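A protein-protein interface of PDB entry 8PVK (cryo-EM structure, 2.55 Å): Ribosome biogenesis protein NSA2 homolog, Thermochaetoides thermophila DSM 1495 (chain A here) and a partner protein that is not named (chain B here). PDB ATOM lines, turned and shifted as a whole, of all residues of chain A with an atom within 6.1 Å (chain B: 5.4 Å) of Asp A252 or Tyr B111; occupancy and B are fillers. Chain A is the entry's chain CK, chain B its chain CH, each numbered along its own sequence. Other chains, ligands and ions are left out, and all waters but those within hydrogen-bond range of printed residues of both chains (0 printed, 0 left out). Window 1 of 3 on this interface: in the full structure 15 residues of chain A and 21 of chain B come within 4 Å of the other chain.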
ATOM      1  N   TYR A 179      18.128  -1.455  -3.098  1.00  0.00           N
ATOM      2  CA  TYR A 179      19.249  -0.719  -2.539  1.00  0.00           C
ATOM      3  C   TYR A 179      20.384  -0.665  -3.550  1.00  0.00           C
ATOM      4  O   TYR A 179      20.588  -1.599  -4.330  1.00  0.00           O
ATOM      5  CB  TYR A 179      19.748  -1.360  -1.236  1.00  0.00           C
ATOM      6  CG  TYR A 179      18.843  -1.122  -0.051  1.00  0.00           C
ATOM      7  CD1 TYR A 179      17.692  -1.877   0.130  1.00  0.00           C
ATOM      8  CD2 TYR A 179      19.137  -0.138   0.884  1.00  0.00           C
ATOM      9  CE1 TYR A 179      16.861  -1.661   1.207  1.00  0.00           C
ATOM     10  CE2 TYR A 179      18.311   0.084   1.966  1.00  0.00           C
ATOM     11  CZ  TYR A 179      17.175  -0.679   2.122  1.00  0.00           C
ATOM     12  OH  TYR A 179      16.347  -0.463   3.197  1.00  0.00           O
ATOM     13  N   ASN A 247      24.598  -7.529   8.662  1.00  0.00           N
ATOM     14  CA  ASN A 247      23.379  -7.122   9.342  1.00  0.00           C
ATOM     15  C   ASN A 247      22.175  -7.745   8.649  1.00  0.00           C
ATOM     16  O   ASN A 247      22.307  -8.499   7.682  1.00  0.00           O
ATOM     17  CB  ASN A 247      23.253  -5.595   9.377  1.00  0.00           C
ATOM     18  CG  ASN A 247      22.856  -5.010   8.036  1.00  0.00           C
ATOM     19  OD1 ASN A 247      23.472  -5.301   7.011  1.00  0.00           O
ATOM     20  ND2 ASN A 247      21.820  -4.183   8.037  1.00  0.00           N
ATOM     21  N   ASN A 248      20.988  -7.412   9.148  1.00  0.00           N
ATOM     22  CA  ASN A 248      19.738  -7.807   8.509  1.00  0.00           C
ATOM     23  C   ASN A 248      19.091  -6.572   7.900  1.00  0.00           C
ATOM     24  O   ASN A 248      18.466  -5.777   8.622  1.00  0.00           O
ATOM     25  CB  ASN A 248      18.795  -8.471   9.517  1.00  0.00           C
ATOM     26  CG  ASN A 248      19.251  -9.861   9.906  1.00  0.00           C
ATOM     27  OD1 ASN A 248      19.255 -10.776   9.085  1.00  0.00           O
ATOM     28  ND2 ASN A 248      19.642 -10.025  11.163  1.00  0.00           N
ATOM     29  N   PRO A 249      19.234  -6.352   6.588  1.00  0.00           N
ATOM     30  CA  PRO A 249      18.666  -5.140   5.977  1.00  0.00           C
ATOM     31  C   PRO A 249      17.150  -5.082   6.024  1.00  0.00           C
ATOM     32  O   PRO A 249      16.596  -3.979   6.102  1.00  0.00           O
ATOM     33  CB  PRO A 249      19.184  -5.199   4.532  1.00  0.00           C
ATOM     34  CG  PRO A 249      20.354  -6.129   4.578  1.00  0.00           C
ATOM     35  CD  PRO A 249      20.016  -7.140   5.624  1.00  0.00           C
ATOM     36  N   GLU A 250      16.465  -6.229   6.000  1.00  0.00           N
ATOM     37  CA  GLU A 250      15.010  -6.235   6.101  1.00  0.00           C
ATOM     38  C   GLU A 250      14.525  -5.784   7.473  1.00  0.00           C
ATOM     39  O   GLU A 250      13.370  -5.367   7.602  1.00  0.00           O
ATOM     40  CB  GLU A 250      14.460  -7.627   5.779  1.00  0.00           C
ATOM     41  CG  GLU A 250      14.594  -8.649   6.897  1.00  0.00           C
ATOM     42  CD  GLU A 250      15.932  -9.365   6.888  1.00  0.00           C
ATOM     43  OE1 GLU A 250      16.763  -9.075   6.002  1.00  0.00           O
ATOM     44  OE2 GLU A 250      16.148 -10.224   7.766  1.00  0.00           O
ATOM     45  N   ASN A 251      15.378  -5.855   8.493  1.00  0.00           N
ATOM     46  CA  ASN A 251      15.040  -5.366   9.821  1.00  0.00           C
ATOM     47  C   ASN A 251      15.580  -3.969  10.081  1.00  0.00           C
ATOM     48  O   ASN A 251      14.995  -3.226  10.877  1.00  0.00           O
ATOM     49  CB  ASN A 251      15.585  -6.318  10.889  1.00  0.00           C
ATOM     50  CG  ASN A 251      14.741  -7.564  11.044  1.00  0.00           C
ATOM     51  OD1 ASN A 251      13.608  -7.624  10.572  1.00  0.00           O
ATOM     52  ND2 ASN A 251      15.292  -8.569  11.712  1.00  0.00           N
ATOM     53  N   ASP A 252      16.677  -3.592   9.427  1.00  0.00           N
ATOM     54  CA  ASP A 252      17.376  -2.356   9.757  1.00  0.00           C
ATOM     55  C   ASP A 252      17.077  -1.202   8.814  1.00  0.00           C
ATOM     56  O   ASP A 252      17.148  -0.043   9.238  1.00  0.00           O
ATOM     57  CB  ASP A 252      18.888  -2.598   9.779  1.00  0.00           C
ATOM     58  CG  ASP A 252      19.307  -3.542  10.883  1.00  0.00           C
ATOM     59  OD1 ASP A 252      18.543  -3.689  11.859  1.00  0.00           O
ATOM     60  OD2 ASP A 252      20.399  -4.137  10.778  1.00  0.00           O
ATOM     61  N   GLY A 253      16.750  -1.472   7.554  1.00  0.00           N
ATOM     62  CA  GLY A 253      16.593  -0.404   6.592  1.00  0.00           C
ATOM     63  C   GLY A 253      17.880   0.089   5.973  1.00  0.00           C
ATOM     64  O   GLY A 253      17.855   1.079   5.234  1.00  0.00           O
ATOM     65  N   CYS A 254      19.003  -0.566   6.254  1.00  0.00           N
ATOM     66  CA  CYS A 254      20.281  -0.217   5.655  1.00  0.00           C
ATOM     67  C   CYS A 254      21.109  -1.484   5.523  1.00  0.00           C
ATOM     68  O   CYS A 254      20.867  -2.480   6.208  1.00  0.00           O
ATOM     69  CB  CYS A 254      21.030   0.833   6.485  1.00  0.00           C
ATOM     70  SG  CYS A 254      21.421   0.309   8.168  1.00  0.00           S
ATOM     71  N   ASN A 256      24.793  -3.126   5.889  1.00  0.00           N
ATOM     72  CA  ASN A 256      26.097  -3.016   6.529  1.00  0.00           C
ATOM     73  C   ASN A 256      26.970  -4.169   6.065  1.00  0.00           C
ATOM     74  O   ASN A 256      26.544  -5.327   6.098  1.00  0.00           O
ATOM     75  CB  ASN A 256      25.967  -3.037   8.053  1.00  0.00           C
ATOM     76  CG  ASN A 256      25.214  -1.842   8.592  1.00  0.00           C
ATOM     77  OD1 ASN A 256      25.211  -0.770   7.989  1.00  0.00           O
ATOM     78  ND2 ASN A 256      24.571  -2.020   9.738  1.00  0.00           N
ATOM     79  N   VAL B  49       5.727   6.134  13.400  1.00  0.00           N
ATOM     80  CA  VAL B  49       6.824   6.812  12.704  1.00  0.00           C
ATOM     81  C   VAL B  49       6.379   8.178  12.186  1.00  0.00           C
ATOM     82  O   VAL B  49       7.092   9.186  12.342  1.00  0.00           O
ATOM     83  CB  VAL B  49       7.357   5.916  11.569  1.00  0.00           C
ATOM     84  CG1 VAL B  49       8.320   6.683  10.670  1.00  0.00           C
ATOM     85  CG2 VAL B  49       8.021   4.676  12.142  1.00  0.00           C
ATOM     86  N   THR B 106      13.024  12.768   5.415  1.00  0.00           N
ATOM     87  CA  THR B 106      13.477  11.754   4.462  1.00  0.00           C
ATOM     88  C   THR B 106      13.510  10.361   5.091  1.00  0.00           C
ATOM     89  O   THR B 106      13.069   9.378   4.472  1.00  0.00           O
ATOM     90  CB  THR B 106      14.856  12.136   3.920  1.00  0.00           C
ATOM     91  OG1 THR B 106      14.764  13.378   3.213  1.00  0.00           O
ATOM     92  CG2 THR B 106      15.385  11.068   2.973  1.00  0.00           C
ATOM     93  N   ILE B 107      14.014  10.259   6.326  1.00  0.00           N
ATOM     94  CA  ILE B 107      14.037   8.975   7.030  1.00  0.00           C
ATOM     95  C   ILE B 107      12.625   8.462   7.279  1.00  0.00           C
ATOM     96  O   ILE B 107      12.357   7.258   7.158  1.00  0.00           O
ATOM     97  CB  ILE B 107      14.850   9.093   8.335  1.00  0.00           C
ATOM     98  CG1 ILE B 107      16.303   9.417   8.016  1.00  0.00           C
ATOM     99  CG2 ILE B 107      14.758   7.842   9.190  1.00  0.00           C
ATOM    100  CD1 ILE B 107      17.101   9.791   9.217  1.00  0.00           C
ATOM    101  N   SER B 108      11.699   9.363   7.620  1.00  0.00           N
ATOM    102  CA  SER B 108      10.315   8.951   7.822  1.00  0.00           C
ATOM    103  C   SER B 108       9.695   8.405   6.543  1.00  0.00           C
ATOM    104  O   SER B 108       8.996   7.385   6.575  1.00  0.00           O
ATOM    105  CB  SER B 108       9.495  10.120   8.339  1.00  0.00           C
ATOM    106  OG  SER B 108       8.183   9.716   8.682  1.00  0.00           O
ATOM    107  N   ARG B 109       9.943   9.070   5.408  1.00  0.00           N
ATOM    108  CA  ARG B 109       9.422   8.577   4.134  1.00  0.00           C
ATOM    109  C   ARG B 109       9.991   7.203   3.793  1.00  0.00           C
ATOM    110  O   ARG B 109       9.246   6.297   3.384  1.00  0.00           O
ATOM    111  CB  ARG B 109       9.731   9.575   3.019  1.00  0.00           C
ATOM    112  CG  ARG B 109       8.769  10.743   2.954  1.00  0.00           C
ATOM    113  CD  ARG B 109       8.942  11.520   1.665  1.00  0.00           C
ATOM    114  NE  ARG B 109      10.306  12.012   1.512  1.00  0.00           N
ATOM    115  CZ  ARG B 109      10.690  13.248   1.801  1.00  0.00           C
ATOM    116  NH1 ARG B 109       9.836  14.148   2.259  1.00  0.00           N
ATOM    117  NH2 ARG B 109      11.964  13.589   1.624  1.00  0.00           N
ATOM    118  N   ASP B 110      11.301   7.020   3.996  1.00  0.00           N
ATOM    119  CA  ASP B 110      11.936   5.739   3.690  1.00  0.00           C
ATOM    120  C   ASP B 110      11.388   4.611   4.560  1.00  0.00           C
ATOM    121  O   ASP B 110      11.084   3.519   4.059  1.00  0.00           O
ATOM    122  CB  ASP B 110      13.450   5.851   3.866  1.00  0.00           C
ATOM    123  CG  ASP B 110      14.112   6.614   2.742  1.00  0.00           C
ATOM    124  OD1 ASP B 110      13.498   6.737   1.661  1.00  0.00           O
ATOM    125  OD2 ASP B 110      15.247   7.096   2.939  1.00  0.00           O
ATOM    126  N   TYR B 111      11.236   4.857   5.861  1.00  0.00           N
ATOM    127  CA  TYR B 111      10.785   3.781   6.736  1.00  0.00           C
ATOM    128  C   TYR B 111       9.288   3.524   6.627  1.00  0.00           C
ATOM    129  O   TYR B 111       8.850   2.398   6.878  1.00  0.00           O
ATOM    130  CB  TYR B 111      11.195   4.069   8.177  1.00  0.00           C
ATOM    131  CG  TYR B 111      12.629   3.672   8.438  1.00  0.00           C
ATOM    132  CD1 TYR B 111      12.961   2.366   8.770  1.00  0.00           C
ATOM    133  CD2 TYR B 111      13.654   4.592   8.304  1.00  0.00           C
ATOM    134  CE1 TYR B 111      14.273   2.000   8.993  1.00  0.00           C
ATOM    135  CE2 TYR B 111      14.967   4.239   8.525  1.00  0.00           C
ATOM    136  CZ  TYR B 111      15.272   2.942   8.869  1.00  0.00           C
ATOM    137  OH  TYR B 111      16.584   2.592   9.086  1.00  0.00           O
ATOM    138  N   VAL B 112       8.491   4.518   6.226  1.00  0.00           N
ATOM    139  CA  VAL B 112       7.097   4.241   5.887  1.00  0.00           C
ATOM    140  C   VAL B 112       7.022   3.365   4.638  1.00  0.00           C
ATOM    141  O   VAL B 112       6.221   2.417   4.568  1.00  0.00           O
ATOM    142  CB  VAL B 112       6.319   5.562   5.727  1.00  0.00           C
ATOM    143  CG1 VAL B 112       5.029   5.361   4.949  1.00  0.00           C
ATOM    144  CG2 VAL B 112       6.011   6.151   7.092  1.00  0.00           C
ATOM    145  N   ARG B 113       7.888   3.637   3.655  1.00  0.00           N
ATOM    146  CA  ARG B 113       7.941   2.799   2.460  1.00  0.00           C
ATOM    147  C   ARG B 113       8.357   1.367   2.792  1.00  0.00           C
ATOM    148  O   ARG B 113       7.858   0.413   2.184  1.00  0.00           O
ATOM    149  CB  ARG B 113       8.895   3.416   1.441  1.00  0.00           C
ATOM    150  CG  ARG B 113       8.711   2.912   0.026  1.00  0.00           C
ATOM    151  CD  ARG B 113       9.599   3.674  -0.939  1.00  0.00           C
ATOM    152  NE  ARG B 113       9.347   5.110  -0.903  1.00  0.00           N
ATOM    153  CZ  ARG B 113      10.231   6.016  -0.508  1.00  0.00           C
ATOM    154  NH1 ARG B 113      11.436   5.667  -0.089  1.00  0.00           N
ATOM    155  NH2 ARG B 113       9.896   7.302  -0.530  1.00  0.00           N
ATOM    156  N   LEU B 114       9.273   1.196   3.749  1.00  0.00           N
ATOM    157  CA  LEU B 114       9.667  -0.155   4.156  1.00  0.00           C
ATOM    158  C   LEU B 114       8.573  -0.846   4.968  1.00  0.00           C
ATOM    159  O   LEU B 114       8.364  -2.064   4.841  1.00  0.00           O
ATOM    160  CB  LEU B 114      10.969  -0.106   4.950  1.00  0.00           C
ATOM    161  CG  LEU B 114      12.181   0.406   4.175  1.00  0.00           C
ATOM    162  CD1 LEU B 114      13.372   0.556   5.096  1.00  0.00           C
ATOM    163  CD2 LEU B 114      12.503  -0.518   3.011  1.00  0.00           C
ATOM    164  N   LEU B 115       7.871  -0.090   5.818  1.00  0.00           N
ATOM    165  CA  LEU B 115       6.760  -0.638   6.583  1.00  0.00           C
ATOM    166  C   LEU B 115       5.597  -1.049   5.693  1.00  0.00           C
ATOM    167  O   LEU B 115       4.777  -1.871   6.114  1.00  0.00           O
ATOM    168  CB  LEU B 115       6.288   0.379   7.622  1.00  0.00           C
ATOM    169  CG  LEU B 115       7.071   0.378   8.936  1.00  0.00           C
ATOM    170  CD1 LEU B 115       6.605   1.492   9.853  1.00  0.00           C
ATOM    171  CD2 LEU B 115       6.944  -0.966   9.618  1.00  0.00           C
ATOM    172  N   LYS B 116       5.502  -0.480   4.487  1.00  0.00           N
ATOM    173  CA  LYS B 116       4.535  -0.977   3.510  1.00  0.00           C
ATOM    174  C   LYS B 116       4.785  -2.438   3.145  1.00  0.00           C
ATOM    175  O   LYS B 116       3.837  -3.170   2.840  1.00  0.00           O
ATOM    176  CB  LYS B 116       4.570  -0.132   2.238  1.00  0.00           C
ATOM    177  CG  LYS B 116       3.968   1.253   2.359  1.00  0.00           C
ATOM    178  CD  LYS B 116       3.531   1.789   0.997  1.00  0.00           C
ATOM    179  CE  LYS B 116       4.552   1.491  -0.096  1.00  0.00           C
ATOM    180  NZ  LYS B 116       4.064   1.897  -1.440  1.00  0.00           N
ATOM    181  N   LEU B 127      11.877  -2.026  12.292  1.00  0.00           N
ATOM    182  CA  LEU B 127      11.921  -0.876  11.391  1.00  0.00           C
ATOM    183  C   LEU B 127      11.503   0.411  12.099  1.00  0.00           C
ATOM    184  O   LEU B 127      12.102   1.473  11.873  1.00  0.00           O
ATOM    185  CB  LEU B 127      11.040  -1.134  10.171  1.00  0.00           C
ATOM    186  CG  LEU B 127      11.571  -2.175   9.184  1.00  0.00           C
ATOM    187  CD1 LEU B 127      10.517  -2.519   8.146  1.00  0.00           C
ATOM    188  CD2 LEU B 127      12.845  -1.682   8.520  1.00  0.00           C
ATOM    189  N   LYS B 128      10.482   0.334  12.959  1.00  0.00           N
ATOM    190  CA  LYS B 128      10.057   1.502  13.727  1.00  0.00           C
ATOM    191  C   LYS B 128      11.160   1.974  14.667  1.00  0.00           C
ATOM    192  O   LYS B 128      11.449   3.178  14.757  1.00  0.00           O
ATOM    193  CB  LYS B 128       8.782   1.164  14.506  1.00  0.00           C
ATOM    194  CG  LYS B 128       8.029   2.351  15.104  1.00  0.00           C
ATOM    195  CD  LYS B 128       8.404   2.613  16.559  1.00  0.00           C
ATOM    196  CE  LYS B 128       8.026   1.450  17.455  1.00  0.00           C
ATOM    197  NZ  LYS B 128       8.357   1.726  18.880  1.00  0.00           N
ATOM    198  N   ALA B 130      14.326   1.429  14.296  1.00  0.00           N
ATOM    199  CA  ALA B 130      15.395   1.967  13.462  1.00  0.00           C
ATOM    200  C   ALA B 130      15.124   3.412  13.067  1.00  0.00           C
ATOM    201  O   ALA B 130      16.020   4.262  13.151  1.00  0.00           O
ATOM    202  CB  ALA B 130      15.581   1.093  12.224  1.00  0.00           C
ATOM    203  N   ALA B 131      13.885   3.710  12.660  1.00  0.00           N
ATOM    204  CA  ALA B 131      13.534   5.073  12.268  1.00  0.00           C
ATOM    205  C   ALA B 131      13.669   6.044  13.438  1.00  0.00           C
ATOM    206  O   ALA B 131      14.305   7.100  13.316  1.00  0.00           O
ATOM    207  CB  ALA B 131      12.113   5.104  11.706  1.00  0.00           C
ATOM    208  N   ARG B 134      17.351   6.591  14.414  1.00  0.00           N
ATOM    209  CA  ARG B 134      18.070   7.467  13.493  1.00  0.00           C
ATOM    210  C   ARG B 134      17.669   8.928  13.681  1.00  0.00           C
ATOM    211  O   ARG B 134      18.524   9.826  13.622  1.00  0.00           O
ATOM    212  CB  ARG B 134      17.840   7.002  12.057  1.00  0.00           C
ATOM    213  CG  ARG B 134      18.594   5.724  11.749  1.00  0.00           C
ATOM    214  CD  ARG B 134      18.359   5.205  10.350  1.00  0.00           C
ATOM    215  NE  ARG B 134      18.844   6.112   9.321  1.00  0.00           N
ATOM    216  CZ  ARG B 134      19.080   5.753   8.067  1.00  0.00           C
ATOM    217  NH1 ARG B 134      18.946   4.498   7.672  1.00  0.00           N
ATOM    218  NH2 ARG B 134      19.459   6.676   7.189  1.00  0.00           N
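OD1 of Asn A248 sits close to OE2 of Glu A250.
The side-chain hydroxyl of Tyr A179 sits at hydrogen-bond distance from the backbone carbonyl oxygen of Gly A253.
The side-chain amide nitrogen (ND2) of Asn A247 lies within hydrogen-bond range of the side-chain carboxylate (OD2) of Asp A252, 3.1 Å away.
OH of Tyr B111 sits at hydrogen-bond distance from NH1 of Arg B134, at 3.3 Å.
Hydrophobic or aromatic side chains of chain A within 4 Å of the printed part of chain B: Tyr A179.
Hydrophobic or aromatic side chains of chain B that line the printed part of chain A: Tyr B111, Leu B114, Leu B127 and Ala B130.
Among the printed residues, no Asp or Glu carboxylate lies within 4 Å of a Lys or Arg side-chain nitrogen of the other chain.
Asp A252 touches two residues of chain B.
Tyr B111 touches two residues of chain A.
Printed residues of chain B within 4 Å of Glu A250: Leu B127 (3.8 Å).
Printed residues of chain B within 4 Å of Gly A253: Tyr B111 and Leu B114.
Of the printed residues of chain B, Asn A251 touches Leu B127.
Printed residues of chain A within 4 Å of Ala B130: Asp A252.
Printed residues of chain B within 4 Å of Tyr A179: Leu B114 (3.7 Å).
The nearest residue of chain B that does not touch Asp A252 is Leu B127 (4.3 Å).
The nearest residue of chain A that does not touch Tyr B111 is Cys A254 (4.9 Å).
The nearest printed residue of chain B that does not touch Asn A251 is Ala B130 (4.6 Å).
Among the printed residues, merely in contact across the chains: Tyr A179 with Leu B114 (3.7 Å), Glu A250 with Leu B127 (3.8 Å), Asn A251 with Leu B127 (3.5 Å), Asp A252 with Ala B130 (3.6 Å), Gly A253 with Tyr B111 (3.9 Å) and Gly A253 with Leu B114 (3.7 Å).
The side-chain hydroxyl of Tyr B111 sits at hydrogen-bond distance from the backbone carbonyl oxygen of Asp A252, at 2.7 Å.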
